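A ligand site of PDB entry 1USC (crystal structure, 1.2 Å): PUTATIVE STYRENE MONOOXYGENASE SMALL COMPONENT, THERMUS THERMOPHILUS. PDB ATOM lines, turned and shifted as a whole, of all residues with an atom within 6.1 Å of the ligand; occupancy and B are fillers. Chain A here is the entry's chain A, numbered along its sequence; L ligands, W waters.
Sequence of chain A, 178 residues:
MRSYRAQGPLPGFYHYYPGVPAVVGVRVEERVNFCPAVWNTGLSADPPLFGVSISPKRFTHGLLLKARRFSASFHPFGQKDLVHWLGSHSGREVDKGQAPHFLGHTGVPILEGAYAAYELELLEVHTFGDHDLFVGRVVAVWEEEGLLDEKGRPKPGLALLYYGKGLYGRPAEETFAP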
ATOM      1  N   PRO A  21      -0.776  -7.650  17.329  1.00  0.00           N
ATOM      2  CA  PRO A  21       0.110  -7.789  16.176  1.00  0.00           C
ATOM      3  C   PRO A  21      -0.154  -9.125  15.470  1.00  0.00           C
ATOM      4  O   PRO A  21      -0.260 -10.161  16.128  1.00  0.00           O
ATOM      5  CB  PRO A  21       1.497  -7.722  16.795  1.00  0.00           C
ATOM      6  CG  PRO A  21       1.300  -8.393  18.115  1.00  0.00           C
ATOM      7  CD  PRO A  21      -0.057  -7.869  18.584  1.00  0.00           C
ATOM      8  N   ASN A  33      10.011 -17.075   6.652  1.00  0.00           N
ATOM      9  CA  ASN A  33      10.244 -15.824   7.369  1.00  0.00           C
ATOM     10  C   ASN A  33       8.980 -15.453   8.125  1.00  0.00           C
ATOM     11  O   ASN A  33       7.878 -15.828   7.728  1.00  0.00           O
ATOM     12  CB  ASN A  33      10.606 -14.708   6.380  1.00  0.00           C
ATOM     13  CG  ASN A  33      11.318 -13.538   7.062  1.00  0.00           C
ATOM     14  OD1 ASN A  33      12.368 -13.715   7.673  1.00  0.00           O
ATOM     15  ND2 ASN A  33      10.743 -12.338   6.940  1.00  0.00           N
ATOM     16  N   PHE A  34       9.157 -14.719   9.232  1.00  0.00           N
ATOM     17  CA  PHE A  34       8.037 -14.251  10.041  1.00  0.00           C
ATOM     18  C   PHE A  34       8.323 -12.818  10.434  1.00  0.00           C
ATOM     19  O   PHE A  34       9.463 -12.434  10.648  1.00  0.00           O
ATOM     20  CB  PHE A  34       7.901 -15.036  11.351  1.00  0.00           C
ATOM     21  CG  PHE A  34       7.639 -16.496  11.165  1.00  0.00           C
ATOM     22  CD1 PHE A  34       8.659 -17.421  11.303  1.00  0.00           C
ATOM     23  CD2 PHE A  34       6.358 -16.940  10.852  1.00  0.00           C
ATOM     24  CE1 PHE A  34       8.418 -18.771  11.140  1.00  0.00           C
ATOM     25  CE2 PHE A  34       6.098 -18.301  10.688  1.00  0.00           C
ATOM     26  CZ  PHE A  34       7.137 -19.215  10.827  1.00  0.00           C
ATOM     27  N   CYS A  35       7.264 -12.004  10.486  1.00  0.00           N
ATOM     28  CA  CYS A  35       7.389 -10.591  10.838  1.00  0.00           C
ATOM     29  C   CYS A  35       6.063 -10.042  11.369  1.00  0.00           C
ATOM     30  O   CYS A  35       5.042 -10.085  10.687  1.00  0.00           O
ATOM     31  CB  CYS A  35       7.883  -9.820   9.592  1.00  0.00           C
ATOM     32  SG  CYS A  35       7.011  -8.317   9.055  1.00  0.00           S
ATOM     33  N   PRO A  36       6.051  -9.529  12.622  1.00  0.00           N
ATOM     34  CA  PRO A  36       4.809  -9.006  13.174  1.00  0.00           C
ATOM     35  C   PRO A  36       4.366  -7.758  12.441  1.00  0.00           C
ATOM     36  O   PRO A  36       5.183  -6.964  11.964  1.00  0.00           O
ATOM     37  CB  PRO A  36       5.166  -8.739  14.630  1.00  0.00           C
ATOM     38  CG  PRO A  36       6.604  -8.368  14.558  1.00  0.00           C
ATOM     39  CD  PRO A  36       7.168  -9.384  13.584  1.00  0.00           C
ATOM     40  N   ALA A  37       3.056  -7.599  12.363  1.00  0.00           N
ATOM     41  CA  ALA A  37       2.457  -6.442  11.730  1.00  0.00           C
ATOM     42  C   ALA A  37       1.318  -5.954  12.604  1.00  0.00           C
ATOM     43  O   ALA A  37       0.284  -6.614  12.700  1.00  0.00           O
ATOM     44  CB  ALA A  37       1.934  -6.816  10.352  1.00  0.00           C
ATOM     45  N   VAL A  38       1.499  -4.814  13.280  1.00  0.00           N
ATOM     46  CA  VAL A  38       0.435  -4.285  14.133  1.00  0.00           C
ATOM     47  C   VAL A  38      -0.568  -3.538  13.252  1.00  0.00           C
ATOM     48  O   VAL A  38      -1.709  -3.280  13.671  1.00  0.00           O
ATOM     49  CB  VAL A  38       0.967  -3.358  15.261  1.00  0.00           C
ATOM     50  CG1 VAL A  38       1.483  -2.052  14.691  1.00  0.00           C
ATOM     51  CG2 VAL A  38      -0.128  -3.111  16.292  1.00  0.00           C
ATOM     52  N   TRP A  39      -0.160  -3.186  12.037  1.00  0.00           N
ATOM     53  CA  TRP A  39      -1.096  -2.530  11.128  1.00  0.00           C
ATOM     54  C   TRP A  39      -1.788  -3.655  10.359  1.00  0.00           C
ATOM     55  O   TRP A  39      -1.341  -4.081   9.290  1.00  0.00           O
ATOM     56  CB  TRP A  39      -0.363  -1.592  10.150  1.00  0.00           C
ATOM     57  CG  TRP A  39       0.094  -0.308  10.785  1.00  0.00           C
ATOM     58  CD1 TRP A  39      -0.022   0.065  12.097  1.00  0.00           C
ATOM     59  CD2 TRP A  39       0.780   0.764  10.121  1.00  0.00           C
ATOM     60  NE1 TRP A  39       0.546   1.299  12.292  1.00  0.00           N
ATOM     61  CE2 TRP A  39       1.044   1.758  11.095  1.00  0.00           C
ATOM     62  CE3 TRP A  39       1.186   0.988   8.798  1.00  0.00           C
ATOM     63  CZ2 TRP A  39       1.699   2.949  10.793  1.00  0.00           C
ATOM     64  CZ3 TRP A  39       1.850   2.180   8.495  1.00  0.00           C
ATOM     65  CH2 TRP A  39       2.098   3.140   9.486  1.00  0.00           C
ATOM     66  N   ASN A  40      -2.871  -4.147  10.957  1.00  0.00           N
ATOM     67  CA  ASN A  40      -3.648  -5.224  10.362  1.00  0.00           C
ATOM     68  C   ASN A  40      -5.105  -4.968  10.722  1.00  0.00           C
ATOM     69  O   ASN A  40      -5.406  -4.260  11.687  1.00  0.00           O
ATOM     70  CB  ASN A  40      -3.185  -6.591  10.885  1.00  0.00           C
ATOM     71  CG  ASN A  40      -3.512  -6.809  12.356  1.00  0.00           C
ATOM     72  OD1 ASN A  40      -4.644  -7.150  12.714  1.00  0.00           O
ATOM     73  ND2 ASN A  40      -2.527  -6.603  13.224  1.00  0.00           N
ATOM     74  N   SER A  53      -0.482  -4.336   6.566  1.00  0.00           N
ATOM     75  CA  SER A  53       0.223  -3.244   5.913  1.00  0.00           C
ATOM     76  C   SER A  53       1.715  -3.410   6.170  1.00  0.00           C
ATOM     77  O   SER A  53       2.187  -3.260   7.300  1.00  0.00           O
ATOM     78  CB  SER A  53      -0.267  -1.907   6.460  1.00  0.00           C
ATOM     79  OG  SER A  53       0.379  -0.822   5.821  1.00  0.00           O
ATOM     80  N   ILE A  54       2.460  -3.696   5.099  1.00  0.00           N
ATOM     81  CA  ILE A  54       3.891  -3.956   5.185  1.00  0.00           C
ATOM     82  C   ILE A  54       4.740  -2.962   4.398  1.00  0.00           C
ATOM     83  O   ILE A  54       4.474  -2.682   3.231  1.00  0.00           O
ATOM     84  CB  ILE A  54       4.201  -5.382   4.649  1.00  0.00           C
ATOM     85  CG1 ILE A  54       3.289  -6.417   5.324  1.00  0.00           C
ATOM     86  CG2 ILE A  54       5.667  -5.717   4.855  1.00  0.00           C
ATOM     87  CD1 ILE A  54       3.468  -6.549   6.821  1.00  0.00           C
ATOM     88  N   SER A  55       5.791  -2.454   5.039  1.00  0.00           N
ATOM     89  CA  SER A  55       6.694  -1.516   4.393  1.00  0.00           C
ATOM     90  C   SER A  55       7.543  -2.219   3.329  1.00  0.00           C
ATOM     91  O   SER A  55       7.974  -3.351   3.522  1.00  0.00           O
ATOM     92  CB  SER A  55       7.634  -0.891   5.421  1.00  0.00           C
ATOM     93  OG  SER A  55       8.730  -0.250   4.782  1.00  0.00           O
ATOM     94  N   LYS A  57      10.365  -1.845   2.816  1.00  0.00           N
ATOM     95  CA  LYS A  57      11.694  -2.004   3.409  1.00  0.00           C
ATOM     96  C   LYS A  57      11.863  -3.352   4.096  1.00  0.00           C
ATOM     97  O   LYS A  57      12.980  -3.764   4.397  1.00  0.00           O
ATOM     98  CB  LYS A  57      11.959  -0.894   4.428  1.00  0.00           C
ATOM     99  CG  LYS A  57      11.992   0.500   3.843  1.00  0.00           C
ATOM    100  CD  LYS A  57      12.197   1.543   4.939  1.00  0.00           C
ATOM    101  CE  LYS A  57      12.191   2.949   4.379  1.00  0.00           C
ATOM    102  NZ  LYS A  57      12.367   3.972   5.454  1.00  0.00           N
ATOM    103  N   ARG A  58      10.752  -4.036   4.377  1.00  0.00           N
ATOM    104  CA  ARG A  58      10.844  -5.328   5.047  1.00  0.00           C
ATOM    105  C   ARG A  58      11.166  -6.446   4.056  1.00  0.00           C
ATOM    106  O   ARG A  58      10.687  -6.434   2.918  1.00  0.00           O
ATOM    107  CB  ARG A  58       9.533  -5.704   5.747  1.00  0.00           C
ATOM    108  CG  ARG A  58       8.828  -4.602   6.520  1.00  0.00           C
ATOM    109  CD  ARG A  58       9.699  -3.901   7.544  1.00  0.00           C
ATOM    110  NE  ARG A  58       8.898  -2.949   8.304  1.00  0.00           N
ATOM    111  CZ  ARG A  58       9.326  -1.784   8.753  1.00  0.00           C
ATOM    112  NH1 ARG A  58      10.571  -1.389   8.525  1.00  0.00           N
ATOM    113  NH2 ARG A  58       8.504  -0.982   9.413  1.00  0.00           N
ATOM    114  N   PHE A  59      11.975  -7.404   4.498  1.00  0.00           N
ATOM    115  CA  PHE A  59      12.339  -8.552   3.672  1.00  0.00           C
ATOM    116  C   PHE A  59      11.035  -9.276   3.313  1.00  0.00           C
ATOM    117  O   PHE A  59      10.877  -9.806   2.212  1.00  0.00           O
ATOM    118  CB  PHE A  59      13.265  -9.459   4.486  1.00  0.00           C
ATOM    119  CG  PHE A  59      13.744 -10.680   3.753  1.00  0.00           C
ATOM    120  CD1 PHE A  59      13.523 -11.951   4.277  1.00  0.00           C
ATOM    121  CD2 PHE A  59      14.460 -10.566   2.565  1.00  0.00           C
ATOM    122  CE1 PHE A  59      14.018 -13.083   3.646  1.00  0.00           C
ATOM    123  CE2 PHE A  59      14.953 -11.696   1.914  1.00  0.00           C
ATOM    124  CZ  PHE A  59      14.733 -12.960   2.459  1.00  0.00           C
ATOM    125  N   THR A  60      10.091  -9.275   4.250  1.00  0.00           N
ATOM    126  CA  THR A  60       8.809  -9.929   4.061  1.00  0.00           C
ATOM    127  C   THR A  60       8.021  -9.400   2.862  1.00  0.00           C
ATOM    128  O   THR A  60       7.297 -10.149   2.206  1.00  0.00           O
ATOM    129  CB  THR A  60       7.948  -9.765   5.337  1.00  0.00           C
ATOM    130  OG1 THR A  60       8.601 -10.405   6.439  1.00  0.00           O
ATOM    131  CG2 THR A  60       6.570 -10.368   5.151  1.00  0.00           C
ATOM    132  N   HIS A  61       8.164  -8.118   2.568  1.00  0.00           N
ATOM    133  CA  HIS A  61       7.443  -7.504   1.457  1.00  0.00           C
ATOM    134  C   HIS A  61       7.709  -8.259   0.154  1.00  0.00           C
ATOM    135  O   HIS A  61       6.774  -8.657  -0.541  1.00  0.00           O
ATOM    136  CB  HIS A  61       7.867  -6.035   1.330  1.00  0.00           C
ATOM    137  CG  HIS A  61       7.075  -5.261   0.326  1.00  0.00           C
ATOM    138  ND1 HIS A  61       7.327  -5.321  -1.024  1.00  0.00           N
ATOM    139  CD2 HIS A  61       6.047  -4.396   0.474  1.00  0.00           C
ATOM    140  CE1 HIS A  61       6.483  -4.530  -1.668  1.00  0.00           C
ATOM    141  NE2 HIS A  61       5.699  -3.960  -0.778  1.00  0.00           N
ATOM    142  N   VAL A  83       7.854 -12.675  19.649  1.00  0.00           N
ATOM    143  CA  VAL A  83       7.242 -11.768  18.691  1.00  0.00           C
ATOM    144  C   VAL A  83       8.110 -10.517  18.544  1.00  0.00           C
ATOM    145  O   VAL A  83       8.372 -10.061  17.423  1.00  0.00           O
ATOM    146  CB  VAL A  83       5.817 -11.379  19.137  1.00  0.00           C
ATOM    147  CG1 VAL A  83       5.268 -10.263  18.253  1.00  0.00           C
ATOM    148  CG2 VAL A  83       4.912 -12.599  19.048  1.00  0.00           C
ATOM    149  N   HIS A  84       8.579  -9.959  19.658  1.00  0.00           N
ATOM    150  CA  HIS A  84       9.417  -8.772  19.575  1.00  0.00           C
ATOM    151  C   HIS A  84      10.723  -9.049  18.829  1.00  0.00           C
ATOM    152  O   HIS A  84      11.186  -8.215  18.048  1.00  0.00           O
ATOM    153  CB  HIS A  84       9.732  -8.227  20.971  1.00  0.00           C
ATOM    154  CG  HIS A  84      10.482  -6.934  20.939  1.00  0.00           C
ATOM    155  ND1 HIS A  84       9.987  -5.801  20.336  1.00  0.00           N
ATOM    156  CD2 HIS A  84      11.703  -6.600  21.423  1.00  0.00           C
ATOM    157  CE1 HIS A  84      10.868  -4.827  20.434  1.00  0.00           C
ATOM    158  NE2 HIS A  84      11.920  -5.285  21.088  1.00  0.00           N
ATOM    159  N   TRP A  85      11.311 -10.214  19.077  1.00  0.00           N
ATOM    160  CA  TRP A  85      12.559 -10.568  18.405  1.00  0.00           C
ATOM    161  C   TRP A  85      12.329 -10.632  16.896  1.00  0.00           C
ATOM    162  O   TRP A  85      13.117 -10.120  16.100  1.00  0.00           O
ATOM    163  CB  TRP A  85      13.080 -11.917  18.906  1.00  0.00           C
ATOM    164  CG  TRP A  85      14.416 -12.296  18.327  1.00  0.00           C
ATOM    165  CD1 TRP A  85      15.639 -11.907  18.778  1.00  0.00           C
ATOM    166  CD2 TRP A  85      14.642 -13.083  17.154  1.00  0.00           C
ATOM    167  NE1 TRP A  85      16.630 -12.395  17.945  1.00  0.00           N
ATOM    168  CE2 TRP A  85      16.045 -13.122  16.948  1.00  0.00           C
ATOM    169  CE3 TRP A  85      13.806 -13.757  16.253  1.00  0.00           C
ATOM    170  CZ2 TRP A  85      16.629 -13.808  15.875  1.00  0.00           C
ATOM    171  CZ3 TRP A  85      14.389 -14.433  15.181  1.00  0.00           C
ATOM    172  CH2 TRP A  85      15.781 -14.457  14.999  1.00  0.00           C
ATOM    173  N   LEU A  86      11.234 -11.267  16.484  1.00  0.00           N
ATOM    174  CA  LEU A  86      10.912 -11.373  15.066  1.00  0.00           C
ATOM    175  C   LEU A  86      10.654 -10.003  14.449  1.00  0.00           C
ATOM    176  O   LEU A  86      10.839  -9.816  13.247  1.00  0.00           O
ATOM    177  CB  LEU A  86       9.675 -12.266  14.873  1.00  0.00           C
ATOM    178  CG  LEU A  86       9.849 -13.741  15.240  1.00  0.00           C
ATOM    179  CD1 LEU A  86       8.490 -14.403  15.268  1.00  0.00           C
ATOM    180  CD2 LEU A  86      10.771 -14.436  14.243  1.00  0.00           C
ATOM    181  N   GLY A  87      10.240  -9.052  15.272  1.00  0.00           N
ATOM    182  CA  GLY A  87       9.981  -7.709  14.772  1.00  0.00           C
ATOM    183  C   GLY A  87      11.152  -6.760  14.958  1.00  0.00           C
ATOM    184  O   GLY A  87      11.013  -5.562  14.713  1.00  0.00           O
ATOM    185  N   SER A  88      12.297  -7.278  15.384  1.00  0.00           N
ATOM    186  CA  SER A  88      13.472  -6.447  15.615  1.00  0.00           C
ATOM    187  C   SER A  88      14.697  -6.922  14.848  1.00  0.00           C
ATOM    188  O   SER A  88      15.798  -6.383  15.014  1.00  0.00           O
ATOM    189  CB  SER A  88      13.803  -6.383  17.117  1.00  0.00           C
ATOM    190  OG  SER A  88      12.698  -5.904  17.866  1.00  0.00           O
ATOM    191  N   HIS A  89      14.512  -7.927  14.008  1.00  0.00           N
ATOM    192  CA  HIS A  89      15.582  -8.491  13.190  1.00  0.00           C
ATOM    193  C   HIS A  89      15.010  -8.787  11.805  1.00  0.00           C
ATOM    194  O   HIS A  89      13.814  -9.067  11.680  1.00  0.00           O
ATOM    195  CB  HIS A  89      16.113  -9.767  13.832  1.00  0.00           C
ATOM    196  CG  HIS A  89      16.750  -9.539  15.172  1.00  0.00           C
ATOM    197  ND1 HIS A  89      18.066  -9.147  15.304  1.00  0.00           N
ATOM    198  CD2 HIS A  89      16.233  -9.602  16.424  1.00  0.00           C
ATOM    199  CE1 HIS A  89      18.332  -8.968  16.593  1.00  0.00           C
ATOM    200  NE2 HIS A  89      17.241  -9.240  17.281  1.00  0.00           N
ATOM    201  N   SER A  90      15.852  -8.725  10.783  1.00  0.00           N
ATOM    202  CA  SER A  90      15.417  -8.961   9.417  1.00  0.00           C
ATOM    203  C   SER A  90      15.891 -10.271   8.814  1.00  0.00           C
ATOM    204  O   SER A  90      16.994 -10.744   9.108  1.00  0.00           O
ATOM    205  CB  SER A  90      15.901  -7.814   8.515  1.00  0.00           C
ATOM    206  OG  SER A  90      15.579  -8.080   7.157  1.00  0.00           O
ATOM    207  N   GLY A  91      15.056 -10.848   7.947  1.00  0.00           N
ATOM    208  CA  GLY A  91      15.399 -12.091   7.281  1.00  0.00           C
ATOM    209  C   GLY A  91      16.584 -11.888   6.355  1.00  0.00           C
ATOM    210  O   GLY A  91      17.140 -12.860   5.852  1.00  0.00           O
ATOM    211  N   ARG A  92      16.955 -10.643   6.121  1.00  0.00           N
ATOM    212  CA  ARG A  92      18.114 -10.333   5.281  1.00  0.00           C
ATOM    213  C   ARG A  92      19.382 -10.692   6.034  1.00  0.00           C
ATOM    214  O   ARG A  92      20.428 -10.912   5.425  1.00  0.00           O
ATOM    215  CB  ARG A  92      18.182  -8.840   4.950  1.00  0.00           C
ATOM    216  CG  ARG A  92      17.164  -8.311   3.960  1.00  0.00           C
ATOM    217  CD  ARG A  92      17.448  -6.835   3.682  1.00  0.00           C
ATOM    218  NE  ARG A  92      17.299  -6.013   4.874  1.00  0.00           N
ATOM    219  CZ  ARG A  92      16.134  -5.582   5.348  1.00  0.00           C
ATOM    220  NH1 ARG A  92      15.013  -5.896   4.718  1.00  0.00           N
ATOM    221  NH2 ARG A  92      16.091  -4.860   6.459  1.00  0.00           N
ATOM    222  N   LYS A  96      14.937 -16.587  10.233  1.00  0.00           N
ATOM    223  CA  LYS A  96      13.870 -16.644  11.211  1.00  0.00           C
ATOM    224  C   LYS A  96      13.057 -17.917  11.048  1.00  0.00           C
ATOM    225  O   LYS A  96      12.188 -18.225  11.857  1.00  0.00           O
ATOM    226  CB  LYS A  96      12.990 -15.397  11.116  1.00  0.00           C
ATOM    227  CG  LYS A  96      13.730 -14.133  11.576  1.00  0.00           C
ATOM    228  CD  LYS A  96      12.812 -12.932  11.791  1.00  0.00           C
ATOM    229  CE  LYS A  96      12.673 -12.080  10.539  1.00  0.00           C
ATOM    230  NZ  LYS A  96      11.816 -10.876  10.771  1.00  0.00           N
ATOM    231  N   HIS A 131       3.671   2.388   2.984  1.00  0.00           N
ATOM    232  CA  HIS A 131       3.412   0.964   3.267  1.00  0.00           C
ATOM    233  C   HIS A 131       2.442   0.429   2.222  1.00  0.00           C
ATOM    234  O   HIS A 131       1.619   1.176   1.682  1.00  0.00           O
ATOM    235  CB  HIS A 131       2.757   0.749   4.640  1.00  0.00           C
ATOM    236  CG  HIS A 131       3.698   0.758   5.798  1.00  0.00           C
ATOM    237  ND1 HIS A 131       4.419   1.879   6.180  1.00  0.00           N
ATOM    238  CD2 HIS A 131       3.990  -0.194   6.712  1.00  0.00           C
ATOM    239  CE1 HIS A 131       5.093   1.607   7.279  1.00  0.00           C
ATOM    240  NE2 HIS A 131       4.860   0.360   7.625  1.00  0.00           N
ATOM    241  N   TYR A 162       0.290  -4.540  21.411  1.00  0.00           N
ATOM    242  CA  TYR A 162       1.459  -3.736  21.113  1.00  0.00           C
ATOM    243  C   TYR A 162       1.098  -2.261  21.194  1.00  0.00           C
ATOM    244  O   TYR A 162       0.095  -1.840  20.613  1.00  0.00           O
ATOM    245  CB  TYR A 162       1.986  -4.057  19.708  1.00  0.00           C
ATOM    246  CG  TYR A 162       3.298  -3.396  19.370  1.00  0.00           C
ATOM    247  CD1 TYR A 162       4.407  -3.522  20.225  1.00  0.00           C
ATOM    248  CD2 TYR A 162       3.460  -2.696  18.177  1.00  0.00           C
ATOM    249  CE1 TYR A 162       5.639  -2.961  19.890  1.00  0.00           C
ATOM    250  CE2 TYR A 162       4.691  -2.134  17.832  1.00  0.00           C
ATOM    251  CZ  TYR A 162       5.772  -2.282  18.686  1.00  0.00           C
ATOM    252  OH  TYR A 162       7.008  -1.769  18.334  1.00  0.00           O
ATOM    253  N   TYR A 168       4.831  -3.486  25.105  1.00  0.00           N
ATOM    254  CA  TYR A 168       3.760  -4.468  25.009  1.00  0.00           C
ATOM    255  C   TYR A 168       2.923  -4.543  26.272  1.00  0.00           C
ATOM    256  O   TYR A 168       3.327  -4.076  27.337  1.00  0.00           O
ATOM    257  CB  TYR A 168       4.312  -5.867  24.733  1.00  0.00           C
ATOM    258  CG  TYR A 168       5.108  -5.979  23.468  1.00  0.00           C
ATOM    259  CD1 TYR A 168       6.400  -5.468  23.385  1.00  0.00           C
ATOM    260  CD2 TYR A 168       4.574  -6.592  22.342  1.00  0.00           C
ATOM    261  CE1 TYR A 168       7.138  -5.556  22.208  1.00  0.00           C
ATOM    262  CE2 TYR A 168       5.294  -6.693  21.165  1.00  0.00           C
ATOM    263  CZ  TYR A 168       6.576  -6.175  21.103  1.00  0.00           C
ATOM    264  OH  TYR A 168       7.306  -6.277  19.946  1.00  0.00           O
HETATM  265  N1  LIG L   1       6.417  -3.497  10.074  1.00  0.00           N
HETATM  266  C1  LIG L   1       5.568  -3.252   9.054  1.00  0.00           C
HETATM  267  O1  LIG L   1       5.833  -3.059   7.858  1.00  0.00           O
HETATM  268  N2  LIG L   1       4.132  -3.220   9.362  1.00  0.00           N
HETATM  269  C2  LIG L   1       3.614  -3.416  10.688  1.00  0.00           C
HETATM  270  O2  LIG L   1       2.383  -3.353  10.773  1.00  0.00           O
HETATM  271  C3  LIG L   1       4.552  -3.668  11.680  1.00  0.00           C
HETATM  272  N3  LIG L   1       4.118  -3.869  12.887  1.00  0.00           N
HETATM  273  C4  LIG L   1       5.006  -4.311  13.898  1.00  0.00           C
HETATM  274  C5  LIG L   1       4.580  -4.744  15.175  1.00  0.00           C
HETATM  275  C6  LIG L   1       5.539  -5.187  16.171  1.00  0.00           C
HETATM  276  C7  LIG L   1       5.050  -5.658  17.528  1.00  0.00           C
HETATM  277  C8  LIG L   1       6.971  -5.188  15.857  1.00  0.00           C
HETATM  278  C9  LIG L   1       7.951  -5.633  16.882  1.00  0.00           C
HETATM  279  C10 LIG L   1       7.402  -4.780  14.617  1.00  0.00           C
HETATM  280  C11 LIG L   1       6.458  -4.317  13.562  1.00  0.00           C
HETATM  281  N4  LIG L   1       6.974  -3.942  12.332  1.00  0.00           N
HETATM  282  C12 LIG L   1       6.048  -3.702  11.357  1.00  0.00           C
HETATM  283  C13 LIG L   1       8.368  -4.032  11.898  1.00  0.00           C
HETATM  284  C14 LIG L   1       8.788  -5.380  11.314  1.00  0.00           C
HETATM  285  O3  LIG L   1       8.151  -6.433  12.017  1.00  0.00           O
HETATM  286  C15 LIG L   1      10.271  -5.414  11.488  1.00  0.00           C
HETATM  287  O4  LIG L   1      10.893  -4.428  10.595  1.00  0.00           O
HETATM  288  C16 LIG L   1      10.894  -6.780  11.090  1.00  0.00           C
HETATM  289  O5  LIG L   1      12.207  -6.852  11.564  1.00  0.00           O
HETATM  290  C17 LIG L   1      10.840  -7.004   9.547  1.00  0.00           C
HETATM  291  O6  LIG L   1      11.408  -8.319   9.331  1.00  0.00           O
HETATM  292  P1  LIG L   1      11.762  -8.749   7.863  1.00  0.00           P
HETATM  293  O7  LIG L   1      10.535  -8.740   7.030  1.00  0.00           O
HETATM  294  O8  LIG L   1      12.813  -7.754   7.274  1.00  0.00           O
HETATM  295  O9  LIG L   1      12.344 -10.151   7.918  1.00  0.00           O
HETATM  296  O   HOH W   1      14.102  -5.217  10.678  1.00  0.00           O
HETATM  297  O   HOH W   2      11.359  -2.079  12.099  1.00  0.00           O
HETATM  298  O   HOH W   3      13.558  -5.227   7.994  1.00  0.00           O
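Water W3 lies within hydrogen-bond range of O8 of the ligand (2.7 Å) and NH2 of Arg 92 (3.0 Å).
Ala 37 touches the ligand. Ile 54 touches the ligand. O of Leu 86 touches O5 of the ligand (3.7 Å). O of Gly 87 touches C15 of the ligand, at 3.3 Å. Ser 88 touches the ligand. NE2 of His 131 touches O1 of the ligand (3.6 Å). Tyr 162 touches the ligand (CG to C7, 3.4 Å). OH of Tyr 168 touches C9 of the ligand, at 3.2 Å. Hydrophobic or aromatic side chains that line the ligand: Pro 36, Ala 37, Val 38, Trp 39, Phe 59, His 131, Tyr 162 and Tyr 168. Within 4 Å of the ligand: Asn 33, Cys 35, Pro 36, Ala 37, Val 38, Trp 39, Ser 53, Ile 54, Ser 55, Arg 58, Phe 59, Thr 60, Leu 86, Gly 87, Ser 88, His 89, Ser 90, Gly 91, Arg 92, Lys 96, His 131, Tyr 162 and Tyr 168.
SG of Cys 35 sits close to OG1 of Thr 60. The backbone carbonyl oxygen (O) of Trp 39 is in hydrogen-bond range of the backbone NH (N) of Ser 53 (2.9 Å). The side-chain amino group (NZ) of Lys 96 sits at hydrogen-bond distance from the backbone carbonyl oxygen (O) of Leu 86, 2.9 Å away. The side-chain amino group (NZ) of Lys 96 sits at hydrogen-bond distance from the backbone carbonyl oxygen (O) of Phe 34 (2.8 Å). The backbone carbonyl oxygen of His 89 is in hydrogen-bond range of the side-chain amino group of Lys 96 (2.8 Å). OG of Ser 90 lies close to N of Arg 92 (3.1 Å). The side-chain hydroxyl (OG) of Ser 88 lies within hydrogen-bond range of the backbone carbonyl oxygen (O) of His 84 (2.8 Å). The side-chain hydroxyl (OG) of Ser 55 sits close to the backbone NH (N) of Lys 57, at 3.0 Å.
The backbone NH (N) of Gly 91 lies within hydrogen-bond range of an oxygen (O9) of the ligand (2.8 Å). A nitrogen (N2) of the ligand is in hydrogen-bond range of the backbone carbonyl oxygen of Ser 53. The side-chain amide nitrogen of Asn 33 lies within hydrogen-bond range of an oxygen (O9) of the ligand (2.9 Å). The side-chain hydroxyl of Ser 90 is in hydrogen-bond range of an oxygen (O8) of the ligand, at 2.8 Å. O2 of the ligand is in hydrogen-bond range of N of Trp 39 (2.8 Å). The backbone carbonyl oxygen of His 89 is in hydrogen-bond range of an oxygen (O5) of the ligand, at 2.7 Å. An oxygen (O3) of the ligand is in hydrogen-bond range of the backbone carbonyl oxygen (O) of Pro 36 (3.0 Å). NZ of Lys 96 lies within salt-bridge range of O9 of the ligand, at 3.0 Å. The side-chain sulfur (SG) of Cys 35 sits at hydrogen-bond distance from an oxygen (O3) of the ligand, 3.7 Å away. The backbone NH (N) of Ser 55 is in hydrogen-bond range of an oxygen (O1) of the ligand, at 2.9 Å. NH1 of Arg 92 lies within salt-bridge range of O8 of the ligand (3.9 Å). The backbone NH (N) of Thr 60 sits at hydrogen-bond distance from an oxygen (O7) of the ligand (2.9 Å). The side-chain hydroxyl (OG1) of Thr 60 lies within hydrogen-bond range of an oxygen (O7) of the ligand (2.6 Å). A nitrogen (N3) of the ligand is in hydrogen-bond range of the backbone NH of Val 38 (2.8 Å). A nitrogen (N1) of the ligand lies within hydrogen-bond range of the guanidinium group of Arg 58. N of Phe 59 is in hydrogen-bond range of O8 of the ligand (2.9 Å).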
